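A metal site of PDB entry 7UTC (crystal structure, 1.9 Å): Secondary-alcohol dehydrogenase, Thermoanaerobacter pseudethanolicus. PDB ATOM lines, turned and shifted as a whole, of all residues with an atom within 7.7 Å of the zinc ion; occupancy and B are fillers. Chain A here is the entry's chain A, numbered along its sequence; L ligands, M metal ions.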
ATOM      1  N   ALA A  35      27.174  27.934 -23.525  1.00  0.00           N
ATOM      2  CA  ALA A  35      26.690  27.368 -22.272  1.00  0.00           C
ATOM      3  C   ALA A  35      25.482  26.473 -22.522  1.00  0.00           C
ATOM      4  O   ALA A  35      24.581  26.856 -23.289  1.00  0.00           O
ATOM      5  CB  ALA A  35      26.310  28.466 -21.278  1.00  0.00           C
ATOM      6  N   PRO A  36      25.426  25.305 -21.886  1.00  0.00           N
ATOM      7  CA  PRO A  36      24.234  24.460 -22.002  1.00  0.00           C
ATOM      8  C   PRO A  36      23.153  24.900 -21.036  1.00  0.00           C
ATOM      9  O   PRO A  36      23.397  25.599 -20.054  1.00  0.00           O
ATOM     10  CB  PRO A  36      24.771  23.075 -21.638  1.00  0.00           C
ATOM     11  CG  PRO A  36      25.783  23.384 -20.586  1.00  0.00           C
ATOM     12  CD  PRO A  36      26.432  24.705 -21.010  1.00  0.00           C
ATOM     13  N   CYS A  37      21.930  24.450 -21.313  1.00  0.00           N
ATOM     14  CA  CYS A  37      20.771  24.841 -20.535  1.00  0.00           C
ATOM     15  C   CYS A  37      19.927  23.629 -20.197  1.00  0.00           C
ATOM     16  O   CYS A  37      19.911  22.640 -20.921  1.00  0.00           O
ATOM     17  CB  CYS A  37      19.898  25.860 -21.286  1.00  0.00           C
ATOM     18  SG  CYS A  37      18.571  26.570 -20.274  1.00  0.00           S
ATOM     19  N   THR A  38      19.218  23.730 -19.072  1.00  0.00           N
ATOM     20  CA  THR A  38      18.265  22.686 -18.708  1.00  0.00           C
ATOM     21  C   THR A  38      17.186  22.527 -19.775  1.00  0.00           C
ATOM     22  O   THR A  38      16.608  21.437 -19.909  1.00  0.00           O
ATOM     23  CB  THR A  38      17.619  23.022 -17.360  1.00  0.00           C
ATOM     24  OG1 THR A  38      18.615  23.569 -16.492  1.00  0.00           O
ATOM     25  CG2 THR A  38      17.045  21.771 -16.722  1.00  0.00           C
ATOM     26  N   SER A  39      16.914  23.586 -20.537  1.00  0.00           N
ATOM     27  CA  SER A  39      15.893  23.522 -21.584  1.00  0.00           C
ATOM     28  C   SER A  39      16.251  22.501 -22.648  1.00  0.00           C
ATOM     29  O   SER A  39      15.369  21.809 -23.182  1.00  0.00           O
ATOM     30  CB  SER A  39      15.689  24.898 -22.212  1.00  0.00           C
ATOM     31  OG  SER A  39      15.296  25.855 -21.232  1.00  0.00           O
ATOM     32  N   ASP A  40      17.543  22.377 -22.985  1.00  0.00           N
ATOM     33  CA  ASP A  40      17.968  21.368 -23.938  1.00  0.00           C
ATOM     34  C   ASP A  40      17.819  19.951 -23.384  1.00  0.00           C
ATOM     35  O   ASP A  40      17.737  18.997 -24.160  1.00  0.00           O
ATOM     36  CB  ASP A  40      19.408  21.621 -24.365  1.00  0.00           C
ATOM     37  CG  ASP A  40      19.525  22.778 -25.357  1.00  0.00           C
ATOM     38  OD1 ASP A  40      18.484  23.348 -25.737  1.00  0.00           O
ATOM     39  OD2 ASP A  40      20.667  23.105 -25.738  1.00  0.00           O
ATOM     40  N   GLY A  58      22.027  24.054 -28.123  1.00  0.00           N
ATOM     41  CA  GLY A  58      22.710  25.201 -27.564  1.00  0.00           C
ATOM     42  C   GLY A  58      22.107  26.517 -28.004  1.00  0.00           C
ATOM     43  O   GLY A  58      21.785  26.703 -29.177  1.00  0.00           O
ATOM     44  N   HIS A  59      21.952  27.448 -27.065  1.00  0.00           N
ATOM     45  CA  HIS A  59      21.360  28.740 -27.428  1.00  0.00           C
ATOM     46  C   HIS A  59      21.948  29.920 -26.659  1.00  0.00           C
ATOM     47  O   HIS A  59      21.430  31.029 -26.805  1.00  0.00           O
ATOM     48  CB  HIS A  59      19.826  28.689 -27.252  1.00  0.00           C
ATOM     49  CG  HIS A  59      19.367  28.146 -25.932  1.00  0.00           C
ATOM     50  ND1 HIS A  59      18.919  26.852 -25.780  1.00  0.00           N
ATOM     51  CD2 HIS A  59      19.256  28.732 -24.720  1.00  0.00           C
ATOM     52  CE1 HIS A  59      18.563  26.655 -24.518  1.00  0.00           C
ATOM     53  NE2 HIS A  59      18.760  27.786 -23.858  1.00  0.00           N
ATOM     54  N   GLU A  60      22.990  29.733 -25.868  1.00  0.00           N
ATOM     55  CA  GLU A  60      23.592  30.811 -25.084  1.00  0.00           C
ATOM     56  C   GLU A  60      25.015  30.988 -25.584  1.00  0.00           C
ATOM     57  O   GLU A  60      25.876  30.136 -25.333  1.00  0.00           O
ATOM     58  CB  GLU A  60      23.573  30.479 -23.593  1.00  0.00           C
ATOM     59  CG  GLU A  60      22.319  29.755 -23.170  1.00  0.00           C
ATOM     60  CD  GLU A  60      22.320  29.418 -21.704  1.00  0.00           C
ATOM     61  OE1 GLU A  60      23.050  30.072 -20.933  1.00  0.00           O
ATOM     62  OE2 GLU A  60      21.584  28.490 -21.308  1.00  0.00           O
ATOM     63  N   ALA A  85      19.258  34.428 -26.629  1.00  0.00           N
ATOM     64  CA  ALA A  85      18.665  33.132 -26.922  1.00  0.00           C
ATOM     65  C   ALA A  85      17.397  33.283 -27.764  1.00  0.00           C
ATOM     66  O   ALA A  85      17.068  32.400 -28.566  1.00  0.00           O
ATOM     67  CB  ALA A  85      18.347  32.386 -25.625  1.00  0.00           C
ATOM     68  N   ILE A  86      16.697  34.396 -27.605  1.00  0.00           N
ATOM     69  CA  ILE A  86      15.476  34.682 -28.346  1.00  0.00           C
ATOM     70  C   ILE A  86      15.850  35.651 -29.464  1.00  0.00           C
ATOM     71  O   ILE A  86      16.234  36.790 -29.197  1.00  0.00           O
ATOM     72  CB  ILE A  86      14.403  35.288 -27.433  1.00  0.00           C
ATOM     73  CG1 ILE A  86      14.245  34.425 -26.173  1.00  0.00           C
ATOM     74  CG2 ILE A  86      13.099  35.483 -28.179  1.00  0.00           C
ATOM     75  CD1 ILE A  86      14.083  32.963 -26.433  1.00  0.00           C
ATOM     76  N   TRP A 110      12.040  32.203 -29.854  1.00  0.00           N
ATOM     77  CA  TRP A 110      13.079  31.245 -29.508  1.00  0.00           C
ATOM     78  C   TRP A 110      13.332  30.355 -30.730  1.00  0.00           C
ATOM     79  O   TRP A 110      12.530  29.481 -31.040  1.00  0.00           O
ATOM     80  CB  TRP A 110      12.654  30.434 -28.294  1.00  0.00           C
ATOM     81  CG  TRP A 110      13.568  29.335 -27.910  1.00  0.00           C
ATOM     82  CD1 TRP A 110      14.904  29.229 -28.204  1.00  0.00           C
ATOM     83  CD2 TRP A 110      13.229  28.164 -27.166  1.00  0.00           C
ATOM     84  NE1 TRP A 110      15.408  28.065 -27.684  1.00  0.00           N
ATOM     85  CE2 TRP A 110      14.399  27.390 -27.042  1.00  0.00           C
ATOM     86  CE3 TRP A 110      12.041  27.698 -26.596  1.00  0.00           C
ATOM     87  CZ2 TRP A 110      14.415  26.176 -26.359  1.00  0.00           C
ATOM     88  CZ3 TRP A 110      12.067  26.492 -25.919  1.00  0.00           C
ATOM     89  CH2 TRP A 110      13.242  25.737 -25.811  1.00  0.00           C
ATOM     90  N   SER A 113      18.014  25.845 -31.164  1.00  0.00           N
ATOM     91  CA  SER A 113      17.721  24.544 -30.549  1.00  0.00           C
ATOM     92  C   SER A 113      16.224  24.345 -30.276  1.00  0.00           C
ATOM     93  O   SER A 113      15.838  23.590 -29.381  1.00  0.00           O
ATOM     94  CB  SER A 113      18.532  24.324 -29.261  1.00  0.00           C
ATOM     95  OG  SER A 113      18.013  25.047 -28.146  1.00  0.00           O
ATOM     96  N   PRO A 149      22.732  36.091 -22.346  1.00  0.00           N
ATOM     97  CA  PRO A 149      21.777  35.665 -23.388  1.00  0.00           C
ATOM     98  C   PRO A 149      20.542  34.936 -22.881  1.00  0.00           C
ATOM     99  O   PRO A 149      19.465  35.085 -23.479  1.00  0.00           O
ATOM    100  CB  PRO A 149      22.643  34.776 -24.268  1.00  0.00           C
ATOM    101  CG  PRO A 149      23.959  35.416 -24.199  1.00  0.00           C
ATOM    102  CD  PRO A 149      24.110  35.765 -22.766  1.00  0.00           C
ATOM    103  N   ASP A 150      20.649  34.161 -21.814  1.00  0.00           N
ATOM    104  CA  ASP A 150      19.537  33.305 -21.415  1.00  0.00           C
ATOM    105  C   ASP A 150      19.238  33.425 -19.928  1.00  0.00           C
ATOM    106  O   ASP A 150      18.106  33.755 -19.544  1.00  0.00           O
ATOM    107  CB  ASP A 150      19.863  31.857 -21.791  1.00  0.00           C
ATOM    108  CG  ASP A 150      18.672  30.924 -21.665  1.00  0.00           C
ATOM    109  OD1 ASP A 150      17.555  31.388 -21.351  1.00  0.00           O
ATOM    110  OD2 ASP A 150      18.858  29.713 -21.884  1.00  0.00           O
ATOM    111  N   MET A 151      20.233  33.158 -19.093  1.00  0.00           N
ATOM    112  CA  MET A 151      20.000  33.083 -17.650  1.00  0.00           C
ATOM    113  C   MET A 151      19.545  34.423 -17.089  1.00  0.00           C
ATOM    114  O   MET A 151      18.584  34.493 -16.325  1.00  0.00           O
ATOM    115  CB  MET A 151      21.265  32.605 -16.950  1.00  0.00           C
ATOM    116  CG  MET A 151      21.735  31.223 -17.388  1.00  0.00           C
ATOM    117  SD  MET A 151      20.525  29.939 -17.042  1.00  0.00           S
ATOM    118  CE  MET A 151      19.769  29.695 -18.656  1.00  0.00           C
ATOM    119  N   THR A 154      16.001  35.587 -18.488  1.00  0.00           N
ATOM    120  CA  THR A 154      14.906  34.770 -17.967  1.00  0.00           C
ATOM    121  C   THR A 154      14.678  35.042 -16.492  1.00  0.00           C
ATOM    122  O   THR A 154      13.531  35.258 -16.061  1.00  0.00           O
ATOM    123  CB  THR A 154      15.202  33.282 -18.177  1.00  0.00           C
ATOM    124  OG1 THR A 154      15.373  33.015 -19.576  1.00  0.00           O
ATOM    125  CG2 THR A 154      14.067  32.455 -17.605  1.00  0.00           C
ATOM    126  N   VAL A 178      18.713  30.089 -13.214  1.00  0.00           N
ATOM    127  CA  VAL A 178      17.603  30.978 -13.536  1.00  0.00           C
ATOM    128  C   VAL A 178      17.052  31.618 -12.266  1.00  0.00           C
ATOM    129  O   VAL A 178      16.873  32.846 -12.184  1.00  0.00           O
ATOM    130  CB  VAL A 178      16.504  30.222 -14.297  1.00  0.00           C
ATOM    131  CG1 VAL A 178      15.222  31.028 -14.344  1.00  0.00           C
ATOM    132  CG2 VAL A 178      16.987  29.882 -15.703  1.00  0.00           C
ATOM    133  N   TYR A 267      10.194  26.057 -17.459  1.00  0.00           N
ATOM    134  CA  TYR A 267       9.848  25.272 -18.636  1.00  0.00           C
ATOM    135  C   TYR A 267       9.405  23.898 -18.148  1.00  0.00           C
ATOM    136  O   TYR A 267      10.230  23.051 -17.788  1.00  0.00           O
ATOM    137  CB  TYR A 267      11.040  25.194 -19.583  1.00  0.00           C
ATOM    138  CG  TYR A 267      10.901  24.335 -20.830  1.00  0.00           C
ATOM    139  CD1 TYR A 267       9.685  23.773 -21.208  1.00  0.00           C
ATOM    140  CD2 TYR A 267      12.010  24.099 -21.635  1.00  0.00           C
ATOM    141  CE1 TYR A 267       9.585  22.989 -22.348  1.00  0.00           C
ATOM    142  CE2 TYR A 267      11.912  23.325 -22.776  1.00  0.00           C
ATOM    143  CZ  TYR A 267      10.706  22.775 -23.125  1.00  0.00           C
ATOM    144  OH  TYR A 267      10.623  22.009 -24.265  1.00  0.00           O
ATOM    145  N   LYS A 346      26.394  26.570 -13.265  1.00  0.00           N
ATOM    146  CA  LYS A 346      26.337  26.776 -14.703  1.00  0.00           C
ATOM    147  C   LYS A 346      27.714  26.593 -15.328  1.00  0.00           C
ATOM    148  O   LYS A 346      28.681  27.252 -14.913  1.00  0.00           O
ATOM    149  CB  LYS A 346      25.798  28.166 -15.018  1.00  0.00           C
ATOM    150  CG  LYS A 346      25.449  28.389 -16.476  1.00  0.00           C
ATOM    151  CD  LYS A 346      24.215  27.595 -16.866  1.00  0.00           C
ATOM    152  CE  LYS A 346      23.630  28.118 -18.163  1.00  0.00           C
ATOM    153  NZ  LYS A 346      22.383  27.384 -18.483  1.00  0.00           N
HETATM  154  S1  LIG L   1      15.011  28.935 -23.142  1.00  0.00           S
HETATM  155  O1  LIG L   1      16.102  27.911 -23.097  1.00  0.00           O
HETATM  156  C1  LIG L   1      15.082  29.808 -24.731  1.00  0.00           C
HETATM  157  C2  LIG L   1      13.389  28.132 -23.218  1.00  0.00           C
HETATM  158  P1  LG2 L   2      17.842  23.867 -12.623  1.00  0.00           P
HETATM  159  O1  LG2 L   2      17.564  22.412 -12.659  1.00  0.00           O
HETATM  160  O2  LG2 L   2      19.312  24.121 -12.574  1.00  0.00           O
HETATM  161  O3  LG2 L   2      17.125  24.503 -11.215  1.00  0.00           O
HETATM  162  C1  LG2 L   2      15.895  23.856 -10.797  1.00  0.00           C
HETATM  163  C2  LG2 L   2      15.676  24.258  -9.329  1.00  0.00           C
HETATM  164  O4  LG2 L   2      14.528  23.781  -8.931  1.00  0.00           O
HETATM  165  C3  LG2 L   2      16.761  23.595  -8.481  1.00  0.00           C
HETATM  166  O5  LG2 L   2      17.456  24.532  -7.772  1.00  0.00           O
HETATM  167  C4  LG2 L   2      15.993  22.664  -7.519  1.00  0.00           C
HETATM  168  O6  LG2 L   2      16.620  22.740  -6.154  1.00  0.00           O
HETATM  169  C5  LG2 L   2      14.790  23.185  -7.474  1.00  0.00           C
HETATM  170  N1  LG2 L   2      13.765  22.166  -7.170  1.00  0.00           N
HETATM  171  C6  LG2 L   2      13.597  20.871  -7.487  1.00  0.00           C
HETATM  172  N2  LG2 L   2      12.453  20.460  -6.922  1.00  0.00           N
HETATM  173  C7  LG2 L   2      11.917  21.506  -6.269  1.00  0.00           C
HETATM  174  C8  LG2 L   2      10.756  21.652  -5.513  1.00  0.00           C
HETATM  175  N3  LG2 L   2       9.635  20.672  -5.144  1.00  0.00           N
HETATM  176  N4  LG2 L   2      10.462  22.798  -4.965  1.00  0.00           N
HETATM  177  C9  LG2 L   2      11.301  23.876  -5.130  1.00  0.00           C
HETATM  178  N5  LG2 L   2      12.435  23.736  -5.855  1.00  0.00           N
HETATM  179  C10 LG2 L   2      12.735  22.557  -6.419  1.00  0.00           C
HETATM  180  O7  LG2 L   2      17.164  24.592 -13.954  1.00  0.00           O
HETATM  181  P2  LG2 L   2      17.525  26.132 -14.521  1.00  0.00           P
HETATM  182  O8  LG2 L   2      18.657  26.074 -15.560  1.00  0.00           O
HETATM  183  O9  LG2 L   2      17.948  27.050 -13.323  1.00  0.00           O
HETATM  184  O10 LG2 L   2      16.169  26.786 -15.207  1.00  0.00           O
HETATM  185  C11 LG2 L   2      14.999  26.824 -14.433  1.00  0.00           C
HETATM  186  C12 LG2 L   2      13.816  26.293 -15.294  1.00  0.00           C
HETATM  187  O11 LG2 L   2      13.393  27.236 -16.099  1.00  0.00           O
HETATM  188  C13 LG2 L   2      14.266  25.115 -16.179  1.00  0.00           C
HETATM  189  O12 LG2 L   2      13.307  24.166 -16.211  1.00  0.00           O
HETATM  190  C14 LG2 L   2      14.462  25.745 -17.586  1.00  0.00           C
HETATM  191  O13 LG2 L   2      14.173  24.739 -18.669  1.00  0.00           O
HETATM  192  C15 LG2 L   2      13.598  26.729 -17.629  1.00  0.00           C
HETATM  193  N6  LG2 L   2      14.085  27.841 -18.462  1.00  0.00           N
HETATM  194  C16 LG2 L   2      13.186  28.745 -18.965  1.00  0.00           C
HETATM  195  C17 LG2 L   2      13.619  29.827 -19.761  1.00  0.00           C
HETATM  196  C18 LG2 L   2      12.594  30.882 -20.348  1.00  0.00           C
HETATM  197  O14 LG2 L   2      12.942  31.665 -21.217  1.00  0.00           O
HETATM  198  N7  LG2 L   2      11.194  30.959 -19.816  1.00  0.00           N
HETATM  199  C19 LG2 L   2      14.952  29.948 -20.017  1.00  0.00           C
HETATM  200  C20 LG2 L   2      15.851  29.044 -19.515  1.00  0.00           C
HETATM  201  C21 LG2 L   2      15.398  27.975 -18.717  1.00  0.00           C
HETATM  202  P3  LG2 L   2      17.949  21.791  -5.836  1.00  0.00           P
HETATM  203  O15 LG2 L   2      17.529  20.615  -4.940  1.00  0.00           O
HETATM  204  O16 LG2 L   2      18.998  22.639  -5.138  1.00  0.00           O
HETATM  205  O17 LG2 L   2      18.501  21.240  -7.131  1.00  0.00           O
HETATM  206 ZN    ZN M   1      17.900  28.086 -21.915  1.00  0.00          ZN
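The side-chain hydroxyl (OG) of Ser 39 lies within hydrogen-bond range of an oxygen (O13) of LG2 L2 (3.0 Å). An oxygen (O8) of LG2 L2 is in hydrogen-bond range of the side-chain hydroxyl of Thr 38, at 2.7 Å. The backbone NH (N) of Val 178 is in hydrogen-bond range of an oxygen (O9) of LG2 L2 (3.1 Å). The side-chain hydroxyl (OG1) of Thr 154 lies close to an oxygen (O14) of LG2 L2.
A ring nitrogen (ND1) of His 59 is in hydrogen-bond range of the side-chain hydroxyl (OG) of Ser 113. The side-chain sulfur (SG) of Cys 37 sits close to the side-chain carboxylate (OE2) of Glu 60, 3.7 Å away. The backbone carbonyl oxygen (O) of Asp 150 is in hydrogen-bond range of the side-chain hydroxyl (OG1) of Thr 154 (2.8 Å). The side-chain sulfur (SG) of Cys 37 lies close to the backbone NH (N) of Ser 39. The backbone NH of Ala 35 sits at hydrogen-bond distance from the backbone carbonyl oxygen of Glu 60 (3.1 Å). OE2 of Glu 60 is in salt-bridge range of NZ of Lys 346 (3.1 Å).
Merely in contact with the zinc ion: Ser 39 and Glu 60. Within 4 Å of the zinc ion: Cys 37, Ser 39, His 59, Glu 60 and Asp 150.
The side-chain carboxylate (OD2) of Asp 150 binds the zinc ion (1.9 Å). The zinc ion is bound by a ring nitrogen (NE2) of His 59, at 2.1 Å. O1 of LIG L1 is bound to the zinc ion (2.2 Å). The zinc ion is bound by SG of Cys 37, 2.3 Å away.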
